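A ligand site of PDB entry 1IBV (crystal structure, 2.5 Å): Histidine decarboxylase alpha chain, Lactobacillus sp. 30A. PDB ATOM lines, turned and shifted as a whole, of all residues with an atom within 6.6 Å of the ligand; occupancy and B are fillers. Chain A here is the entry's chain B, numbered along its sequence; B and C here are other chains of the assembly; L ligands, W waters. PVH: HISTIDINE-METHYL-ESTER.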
ATOM      1  C   PYR A   1      32.065  17.191 -12.896  1.00  0.00           C
ATOM      2  O   PYR A   1      32.070  17.997 -13.829  1.00  0.00           O
ATOM      3  CA  PYR A   1      30.920  16.371 -12.777  1.00  0.00           C
ATOM      4  CB  PYR A   1      30.834  15.356 -11.630  1.00  0.00           C
ATOM      5  N   PHE A   2      33.106  17.087 -12.075  1.00  0.00           N
ATOM      6  CA  PHE A   2      34.250  17.967 -12.234  1.00  0.00           C
ATOM      7  C   PHE A   2      35.651  17.368 -12.192  1.00  0.00           C
ATOM      8  O   PHE A   2      35.872  16.249 -11.719  1.00  0.00           O
ATOM      9  CB  PHE A   2      34.169  19.086 -11.205  1.00  0.00           C
ATOM     10  CG  PHE A   2      32.882  19.830 -11.241  1.00  0.00           C
ATOM     11  CD1 PHE A   2      32.803  21.060 -11.863  1.00  0.00           C
ATOM     12  CD2 PHE A   2      31.744  19.292 -10.666  1.00  0.00           C
ATOM     13  CE1 PHE A   2      31.596  21.753 -11.920  1.00  0.00           C
ATOM     14  CE2 PHE A   2      30.544  19.961 -10.718  1.00  0.00           C
ATOM     15  CZ  PHE A   2      30.464  21.191 -11.340  1.00  0.00           C
ATOM     16  N   CYS A  71      34.144   7.125 -11.819  1.00  0.00           N
ATOM     17  CA  CYS A  71      33.885   7.789 -13.080  1.00  0.00           C
ATOM     18  C   CYS A  71      32.731   8.750 -12.995  1.00  0.00           C
ATOM     19  O   CYS A  71      31.756   8.486 -12.286  1.00  0.00           O
ATOM     20  CB  CYS A  71      33.559   6.752 -14.152  1.00  0.00           C
ATOM     21  SG  CYS A  71      34.832   5.523 -14.480  1.00  0.00           S
ATOM     22  N   ALA A  72      32.860   9.896 -13.649  1.00  0.00           N
ATOM     23  CA  ALA A  72      31.760  10.855 -13.692  1.00  0.00           C
ATOM     24  C   ALA A  72      31.002  10.225 -14.851  1.00  0.00           C
ATOM     25  O   ALA A  72      31.334  10.462 -16.019  1.00  0.00           O
ATOM     26  CB  ALA A  72      32.268  12.235 -14.064  1.00  0.00           C
ATOM     27  N   ASN A  73      30.092   9.315 -14.532  1.00  0.00           N
ATOM     28  CA  ASN A  73      29.341   8.627 -15.572  1.00  0.00           C
ATOM     29  C   ASN A  73      27.836   8.766 -15.488  1.00  0.00           C
ATOM     30  O   ASN A  73      27.277   9.124 -14.453  1.00  0.00           O
ATOM     31  CB  ASN A  73      29.720   7.146 -15.609  1.00  0.00           C
ATOM     32  CG  ASN A  73      29.279   6.416 -14.372  1.00  0.00           C
ATOM     33  OD1 ASN A  73      29.946   6.446 -13.345  1.00  0.00           O
ATOM     34  ND2 ASN A  73      28.134   5.764 -14.452  1.00  0.00           N
ATOM     35  N   LYS A  74      27.192   8.506 -16.622  1.00  0.00           N
ATOM     36  CA  LYS A  74      25.752   8.557 -16.757  1.00  0.00           C
ATOM     37  C   LYS A  74      25.426   7.606 -17.910  1.00  0.00           C
ATOM     38  O   LYS A  74      26.342   7.092 -18.570  1.00  0.00           O
ATOM     39  CB  LYS A  74      25.298   9.974 -17.106  1.00  0.00           C
ATOM     40  CG  LYS A  74      24.390  10.600 -16.070  1.00  0.00           C
ATOM     41  CD  LYS A  74      24.775  12.032 -15.766  1.00  0.00           C
ATOM     42  CE  LYS A  74      23.979  12.553 -14.585  1.00  0.00           C
ATOM     43  NZ  LYS A  74      24.782  13.488 -13.746  1.00  0.00           N
ATOM     44  N   ALA A 100      30.735  16.403 -22.306  1.00  0.00           N
ATOM     45  CA  ALA A 100      31.279  17.720 -22.557  1.00  0.00           C
ATOM     46  C   ALA A 100      32.233  18.198 -21.468  1.00  0.00           C
ATOM     47  O   ALA A 100      31.856  18.253 -20.294  1.00  0.00           O
ATOM     48  CB  ALA A 100      30.166  18.714 -22.718  1.00  0.00           C
ATOM     49  N   MET A 113      34.727  21.635 -15.797  1.00  0.00           N
ATOM     50  CA  MET A 113      33.474  20.905 -15.630  1.00  0.00           C
ATOM     51  C   MET A 113      33.087  19.953 -16.747  1.00  0.00           C
ATOM     52  O   MET A 113      33.325  20.209 -17.930  1.00  0.00           O
ATOM     53  CB  MET A 113      32.356  21.930 -15.432  1.00  0.00           C
ATOM     54  CG  MET A 113      30.970  21.368 -15.219  1.00  0.00           C
ATOM     55  SD  MET A 113      29.841  22.735 -14.917  1.00  0.00           S
ATOM     56  CE  MET A 113      29.920  23.566 -16.508  1.00  0.00           C
ATOM     57  N   PHE A 114      32.499  18.850 -16.337  1.00  0.00           N
ATOM     58  CA  PHE A 114      32.003  17.821 -17.221  1.00  0.00           C
ATOM     59  C   PHE A 114      30.490  17.911 -17.094  1.00  0.00           C
ATOM     60  O   PHE A 114      29.948  18.034 -15.988  1.00  0.00           O
ATOM     61  CB  PHE A 114      32.389  16.425 -16.711  1.00  0.00           C
ATOM     62  CG  PHE A 114      33.735  15.966 -17.141  1.00  0.00           C
ATOM     63  CD1 PHE A 114      34.026  15.806 -18.487  1.00  0.00           C
ATOM     64  CD2 PHE A 114      34.686  15.624 -16.191  1.00  0.00           C
ATOM     65  CE1 PHE A 114      35.258  15.302 -18.874  1.00  0.00           C
ATOM     66  CE2 PHE A 114      35.918  15.120 -16.578  1.00  0.00           C
ATOM     67  CZ  PHE A 114      36.205  14.965 -17.916  1.00  0.00           C
ATOM     68  N   VAL A 115      29.812  17.881 -18.241  1.00  0.00           N
ATOM     69  CA  VAL A 115      28.366  17.899 -18.306  1.00  0.00           C
ATOM     70  C   VAL A 115      28.045  16.745 -19.248  1.00  0.00           C
ATOM     71  O   VAL A 115      28.554  16.707 -20.374  1.00  0.00           O
ATOM     72  CB  VAL A 115      27.811  19.208 -18.897  1.00  0.00           C
ATOM     73  CG1 VAL A 115      26.340  19.053 -19.217  1.00  0.00           C
ATOM     74  CG2 VAL A 115      27.996  20.344 -17.902  1.00  0.00           C
ATOM     75  N   GLU A 116      27.280  15.771 -18.758  1.00  0.00           N
ATOM     76  CA  GLU A 116      26.940  14.621 -19.583  1.00  0.00           C
ATOM     77  C   GLU A 116      25.436  14.577 -19.850  1.00  0.00           C
ATOM     78  O   GLU A 116      24.634  15.048 -19.035  1.00  0.00           O
ATOM     79  CB  GLU A 116      27.413  13.326 -18.923  1.00  0.00           C
ATOM     80  CG  GLU A 116      28.859  13.351 -18.478  1.00  0.00           C
ATOM     81  CD  GLU A 116      29.328  12.013 -17.970  1.00  0.00           C
ATOM     82  OE1 GLU A 116      28.552  11.312 -17.294  1.00  0.00           O
ATOM     83  OE2 GLU A 116      30.485  11.643 -18.248  1.00  0.00           O
ATOM     84  N   ASP A 117      25.071  13.993 -20.980  1.00  0.00           N
ATOM     85  CA  ASP A 117      23.683  13.900 -21.393  1.00  0.00           C
ATOM     86  C   ASP A 117      23.478  12.566 -22.102  1.00  0.00           C
ATOM     87  O   ASP A 117      24.434  11.976 -22.593  1.00  0.00           O
ATOM     88  CB  ASP A 117      23.358  15.059 -22.358  1.00  0.00           C
ATOM     89  CG  ASP A 117      21.861  15.338 -22.489  1.00  0.00           C
ATOM     90  OD1 ASP A 117      21.496  16.142 -23.379  1.00  0.00           O
ATOM     91  OD2 ASP A 117      21.061  14.791 -21.695  1.00  0.00           O
ATOM     92  N   CYS A 147      25.447  26.507 -15.465  1.00  0.00           N
ATOM     93  CA  CYS A 147      26.189  25.984 -14.311  1.00  0.00           C
ATOM     94  C   CYS A 147      27.310  26.953 -13.927  1.00  0.00           C
ATOM     95  O   CYS A 147      27.488  27.250 -12.743  1.00  0.00           O
ATOM     96  CB  CYS A 147      26.754  24.581 -14.597  1.00  0.00           C
ATOM     97  SG  CYS A 147      25.600  23.189 -14.312  1.00  0.00           S
ATOM     98  N   THR A 177      28.079   7.463 -21.153  1.00  0.00           N
ATOM     99  CA  THR A 177      28.976   8.607 -21.224  1.00  0.00           C
ATOM    100  C   THR A 177      29.775   8.537 -19.933  1.00  0.00           C
ATOM    101  O   THR A 177      29.199   8.589 -18.833  1.00  0.00           O
ATOM    102  CB  THR A 177      28.207   9.932 -21.321  1.00  0.00           C
ATOM    103  OG1 THR A 177      29.109  11.020 -21.124  1.00  0.00           O
ATOM    104  CG2 THR A 177      27.106  10.001 -20.287  1.00  0.00           C
ATOM    105  N   TYR A 181      38.792   8.485 -13.811  1.00  0.00           N
ATOM    106  CA  TYR A 181      39.823   9.208 -13.077  1.00  0.00           C
ATOM    107  C   TYR A 181      40.857   8.179 -12.686  1.00  0.00           C
ATOM    108  O   TYR A 181      40.647   7.400 -11.760  1.00  0.00           O
ATOM    109  CB  TYR A 181      39.232   9.865 -11.831  1.00  0.00           C
ATOM    110  CG  TYR A 181      38.287  11.001 -12.151  1.00  0.00           C
ATOM    111  CD1 TYR A 181      37.027  10.751 -12.710  1.00  0.00           C
ATOM    112  CD2 TYR A 181      38.678  12.318 -11.960  1.00  0.00           C
ATOM    113  CE1 TYR A 181      36.187  11.802 -13.055  1.00  0.00           C
ATOM    114  CE2 TYR A 181      37.838  13.369 -12.305  1.00  0.00           C
ATOM    115  CZ  TYR A 181      36.605  13.103 -12.854  1.00  0.00           C
ATOM    116  OH  TYR A 181      35.808  14.163 -13.211  1.00  0.00           O
ATOM    117  N   THR B  79      30.461   5.686  -9.194  1.00  0.00           N
ATOM    118  CA  THR B  79      29.856   6.847  -9.800  1.00  0.00           C
ATOM    119  C   THR B  79      30.020   8.171  -9.065  1.00  0.00           C
ATOM    120  O   THR B  79      29.809   8.264  -7.868  1.00  0.00           O
ATOM    121  CB  THR B  79      28.357   6.590 -10.078  1.00  0.00           C
ATOM    122  OG1 THR B  79      28.227   5.435 -10.909  1.00  0.00           O
ATOM    123  CG2 THR B  79      27.714   7.771 -10.778  1.00  0.00           C
ATOM    124  N   ALA B  80      30.386   9.188  -9.835  1.00  0.00           N
ATOM    125  CA  ALA B  80      30.568  10.527  -9.330  1.00  0.00           C
ATOM    126  C   ALA B  80      29.580  11.357 -10.144  1.00  0.00           C
ATOM    127  O   ALA B  80      29.485  11.177 -11.354  1.00  0.00           O
ATOM    128  CB  ALA B  80      31.985  11.000  -9.573  1.00  0.00           C
ATOM    129  N   SER B  81      28.863  12.260  -9.484  1.00  0.00           N
ATOM    130  CA  SER B  81      27.877  13.088 -10.156  1.00  0.00           C
ATOM    131  C   SER B  81      27.882  14.541  -9.714  1.00  0.00           C
ATOM    132  O   SER B  81      27.344  15.367 -10.467  1.00  0.00           O
ATOM    133  CB  SER B  81      26.480  12.491  -9.949  1.00  0.00           C
ATOM    134  OG  SER B  81      26.348  11.963  -8.644  1.00  0.00           O
ATOM    135  OXT SER B  81      28.425  14.855  -8.635  1.00  0.00           O
ATOM    136  N   ILE C  59      20.591  18.034 -13.934  1.00  0.00           N
ATOM    137  CA  ILE C  59      21.951  18.518 -13.712  1.00  0.00           C
ATOM    138  C   ILE C  59      21.961  19.934 -13.131  1.00  0.00           C
ATOM    139  O   ILE C  59      22.440  20.156 -12.019  1.00  0.00           O
ATOM    140  CB  ILE C  59      22.753  18.545 -15.031  1.00  0.00           C
ATOM    141  CG1 ILE C  59      22.865  17.137 -15.629  1.00  0.00           C
ATOM    142  CG2 ILE C  59      24.146  19.133 -14.787  1.00  0.00           C
ATOM    143  CD1 ILE C  59      23.782  16.213 -14.874  1.00  0.00           C
ATOM    144  N   TYR C  62      20.251  20.404  -9.825  1.00  0.00           N
ATOM    145  CA  TYR C  62      21.069  19.721  -8.838  1.00  0.00           C
ATOM    146  C   TYR C  62      22.407  20.445  -8.694  1.00  0.00           C
ATOM    147  O   TYR C  62      23.295  19.980  -7.985  1.00  0.00           O
ATOM    148  CB  TYR C  62      21.272  18.269  -9.264  1.00  0.00           C
ATOM    149  CG  TYR C  62      22.371  17.510  -8.575  1.00  0.00           C
ATOM    150  CD1 TYR C  62      22.230  17.073  -7.257  1.00  0.00           C
ATOM    151  CD2 TYR C  62      23.565  17.211  -9.241  1.00  0.00           C
ATOM    152  CE1 TYR C  62      23.229  16.335  -6.625  1.00  0.00           C
ATOM    153  CE2 TYR C  62      24.568  16.481  -8.638  1.00  0.00           C
ATOM    154  CZ  TYR C  62      24.401  16.042  -7.330  1.00  0.00           C
ATOM    155  OH  TYR C  62      25.390  15.282  -6.727  1.00  0.00           O
ATOM    156  N   ASP C  63      22.536  21.592  -9.349  1.00  0.00           N
ATOM    157  CA  ASP C  63      23.763  22.378  -9.294  1.00  0.00           C
ATOM    158  C   ASP C  63      23.414  23.664  -8.557  1.00  0.00           C
ATOM    159  O   ASP C  63      24.190  24.153  -7.744  1.00  0.00           O
ATOM    160  CB  ASP C  63      24.252  22.680 -10.716  1.00  0.00           C
ATOM    161  CG  ASP C  63      25.691  23.183 -10.739  1.00  0.00           C
ATOM    162  OD1 ASP C  63      26.618  22.358 -10.809  1.00  0.00           O
ATOM    163  OD2 ASP C  63      25.897  24.422 -10.706  1.00  0.00           O
ATOM    164  N   GLU C  66      23.392  22.701  -4.995  1.00  0.00           N
ATOM    165  CA  GLU C  66      24.714  22.513  -4.415  1.00  0.00           C
ATOM    166  C   GLU C  66      25.337  23.861  -4.104  1.00  0.00           C
ATOM    167  O   GLU C  66      26.138  23.985  -3.168  1.00  0.00           O
ATOM    168  CB  GLU C  66      25.636  21.768  -5.380  1.00  0.00           C
ATOM    169  CG  GLU C  66      25.261  20.328  -5.636  1.00  0.00           C
ATOM    170  CD  GLU C  66      26.309  19.601  -6.482  1.00  0.00           C
ATOM    171  OE1 GLU C  66      26.803  18.557  -6.027  1.00  0.00           O
ATOM    172  OE2 GLU C  66      26.636  20.073  -7.588  1.00  0.00           O
ATOM    173  N   GLY C  73      29.729  23.662  -4.453  1.00  0.00           N
ATOM    174  CA  GLY C  73      29.650  23.866  -5.882  1.00  0.00           C
ATOM    175  C   GLY C  73      30.259  22.913  -6.887  1.00  0.00           C
ATOM    176  O   GLY C  73      29.530  22.205  -7.575  1.00  0.00           O
ATOM    177  N   GLN C  74      31.574  22.934  -7.046  1.00  0.00           N
ATOM    178  CA  GLN C  74      32.222  22.093  -8.044  1.00  0.00           C
ATOM    179  C   GLN C  74      32.816  20.832  -7.442  1.00  0.00           C
ATOM    180  O   GLN C  74      34.009  20.566  -7.555  1.00  0.00           O
ATOM    181  CB  GLN C  74      33.286  22.891  -8.796  1.00  0.00           C
ATOM    182  CG  GLN C  74      32.721  24.123  -9.468  1.00  0.00           C
ATOM    183  CD  GLN C  74      33.797  24.951 -10.121  1.00  0.00           C
ATOM    184  OE1 GLN C  74      34.692  25.438  -9.444  1.00  0.00           O
ATOM    185  NE2 GLN C  74      33.733  25.086 -11.434  1.00  0.00           N
ATOM    186  N   ILE C  75      31.938  20.042  -6.842  1.00  0.00           N
ATOM    187  CA  ILE C  75      32.328  18.818  -6.175  1.00  0.00           C
ATOM    188  C   ILE C  75      31.940  17.574  -6.948  1.00  0.00           C
ATOM    189  O   ILE C  75      30.941  17.558  -7.659  1.00  0.00           O
ATOM    190  CB  ILE C  75      31.668  18.801  -4.774  1.00  0.00           C
ATOM    191  CG1 ILE C  75      32.606  19.463  -3.774  1.00  0.00           C
ATOM    192  CG2 ILE C  75      31.244  17.406  -4.343  1.00  0.00           C
ATOM    193  CD1 ILE C  75      32.981  20.910  -4.146  1.00  0.00           C
ATOM    194  N   ASN C  76      32.767  16.543  -6.851  1.00  0.00           N
ATOM    195  CA  ASN C  76      32.446  15.279  -7.491  1.00  0.00           C
ATOM    196  C   ASN C  76      31.763  14.513  -6.388  1.00  0.00           C
ATOM    197  O   ASN C  76      32.423  13.982  -5.494  1.00  0.00           O
ATOM    198  CB  ASN C  76      33.710  14.542  -7.916  1.00  0.00           C
ATOM    199  CG  ASN C  76      34.317  15.131  -9.153  1.00  0.00           C
ATOM    200  OD1 ASN C  76      33.764  15.019 -10.242  1.00  0.00           O
ATOM    201  ND2 ASN C  76      35.465  15.756  -9.003  1.00  0.00           N
HETATM  202  N   PVH L   1      29.965  16.471 -13.660  1.00  0.00           N
HETATM  203  CA  PVH L   1      28.786  15.632 -13.530  1.00  0.00           C
HETATM  204  C   PVH L   1      28.594  14.894 -14.840  1.00  0.00           C
HETATM  205  O   PVH L   1      28.562  15.543 -15.890  1.00  0.00           O
HETATM  206  CB  PVH L   1      27.510  16.507 -13.418  1.00  0.00           C
HETATM  207  CG  PVH L   1      27.637  17.760 -12.589  1.00  0.00           C
HETATM  208  ND1 PVH L   1      27.254  17.824 -11.271  1.00  0.00           N
HETATM  209  CD2 PVH L   1      27.897  19.032 -12.961  1.00  0.00           C
HETATM  210  CE1 PVH L   1      27.262  19.081 -10.854  1.00  0.00           C
HETATM  211  NE2 PVH L   1      27.656  19.829 -11.869  1.00  0.00           N
HETATM  212  OXT PVH L   1      28.711  13.535 -14.958  1.00  0.00           O
HETATM  213  CM  PVH L   1      28.093  12.680 -13.946  1.00  0.00           C
HETATM  214  O   HOH W   1      26.299  10.498 -12.179  1.00  0.00           O
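Phe 2 touches the ligand (CE2 to NE2, 3.1 Å).
Ala 72 touches the ligand (CB to OXT, 3.9 Å).
Asn 73 of chain A touches the ligand (O to CM, 3.7 Å).
NZ of Lys 74 of chain A touches CM of the ligand, 3.4 Å away.
Val 115 touches the ligand (CA to O, 3.4 Å).
Ala 80 of chain B touches the ligand (O to CM, 3.3 Å).
Tyr 62 of chain C touches the ligand (CE2 to ND1, 3.99 Å).
Glu 66 of chain C touches the ligand (OE2 to CE1, 3.5 Å).
Of the 26 residues printed, 13 come within 4 Å of the ligand.
The nearest printed residue that does not touch the ligand is Ile 59 of chain C (4.01 Å).
O of PYR 1 lies close to N of the ligand (2.6 Å).
A nitrogen (ND1) of the ligand sits at hydrogen-bond distance from the chain-end carboxylate (O) of Ser 81 of chain B (2.6 Å).
O of Phe 114 lies within hydrogen-bond range of N of the ligand, 2.8 Å away.
The side-chain carboxylate (OD1) of Asp 63 of chain C sits at hydrogen-bond distance from a nitrogen (NE2) of the ligand.
N of Glu 116 sits at hydrogen-bond distance from O of the ligand, at 3.1 Å.
O of PYR 1 lies within hydrogen-bond range of the backbone NH (N) of Phe 114.
The backbone carbonyl oxygen (O) of Phe 2 sits at hydrogen-bond distance from the side-chain amide nitrogen (ND2) of Asn 76 of chain C, 2.8 Å away.
O of Phe 2 sits at hydrogen-bond distance from OH of Tyr 181, at 2.6 Å.
The side-chain carboxylate of Glu 116 is in hydrogen-bond range of the backbone NH of Lys 74 of chain A (3.2 Å).
The backbone NH (N) of Ala 80 of chain B sits at hydrogen-bond distance from the backbone carbonyl oxygen (O) of Cys 71.
N of Val 115 lies within hydrogen-bond range of O of Ala 100 (2.9 Å).
O of Thr 177 sits at hydrogen-bond distance from N of Lys 74 of chain A, at 3.0 Å.
The side-chain amide oxygen of Asn 73 of chain A is in hydrogen-bond range of the side-chain hydroxyl of Thr 79 of chain B (3.1 Å).
Water W1 lies within hydrogen-bond range of the backbone carbonyl oxygen of Asn 73 of chain A (2.8 Å) and the backbone carbonyl oxygen of Ala 80 of chain B (3.4 Å).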
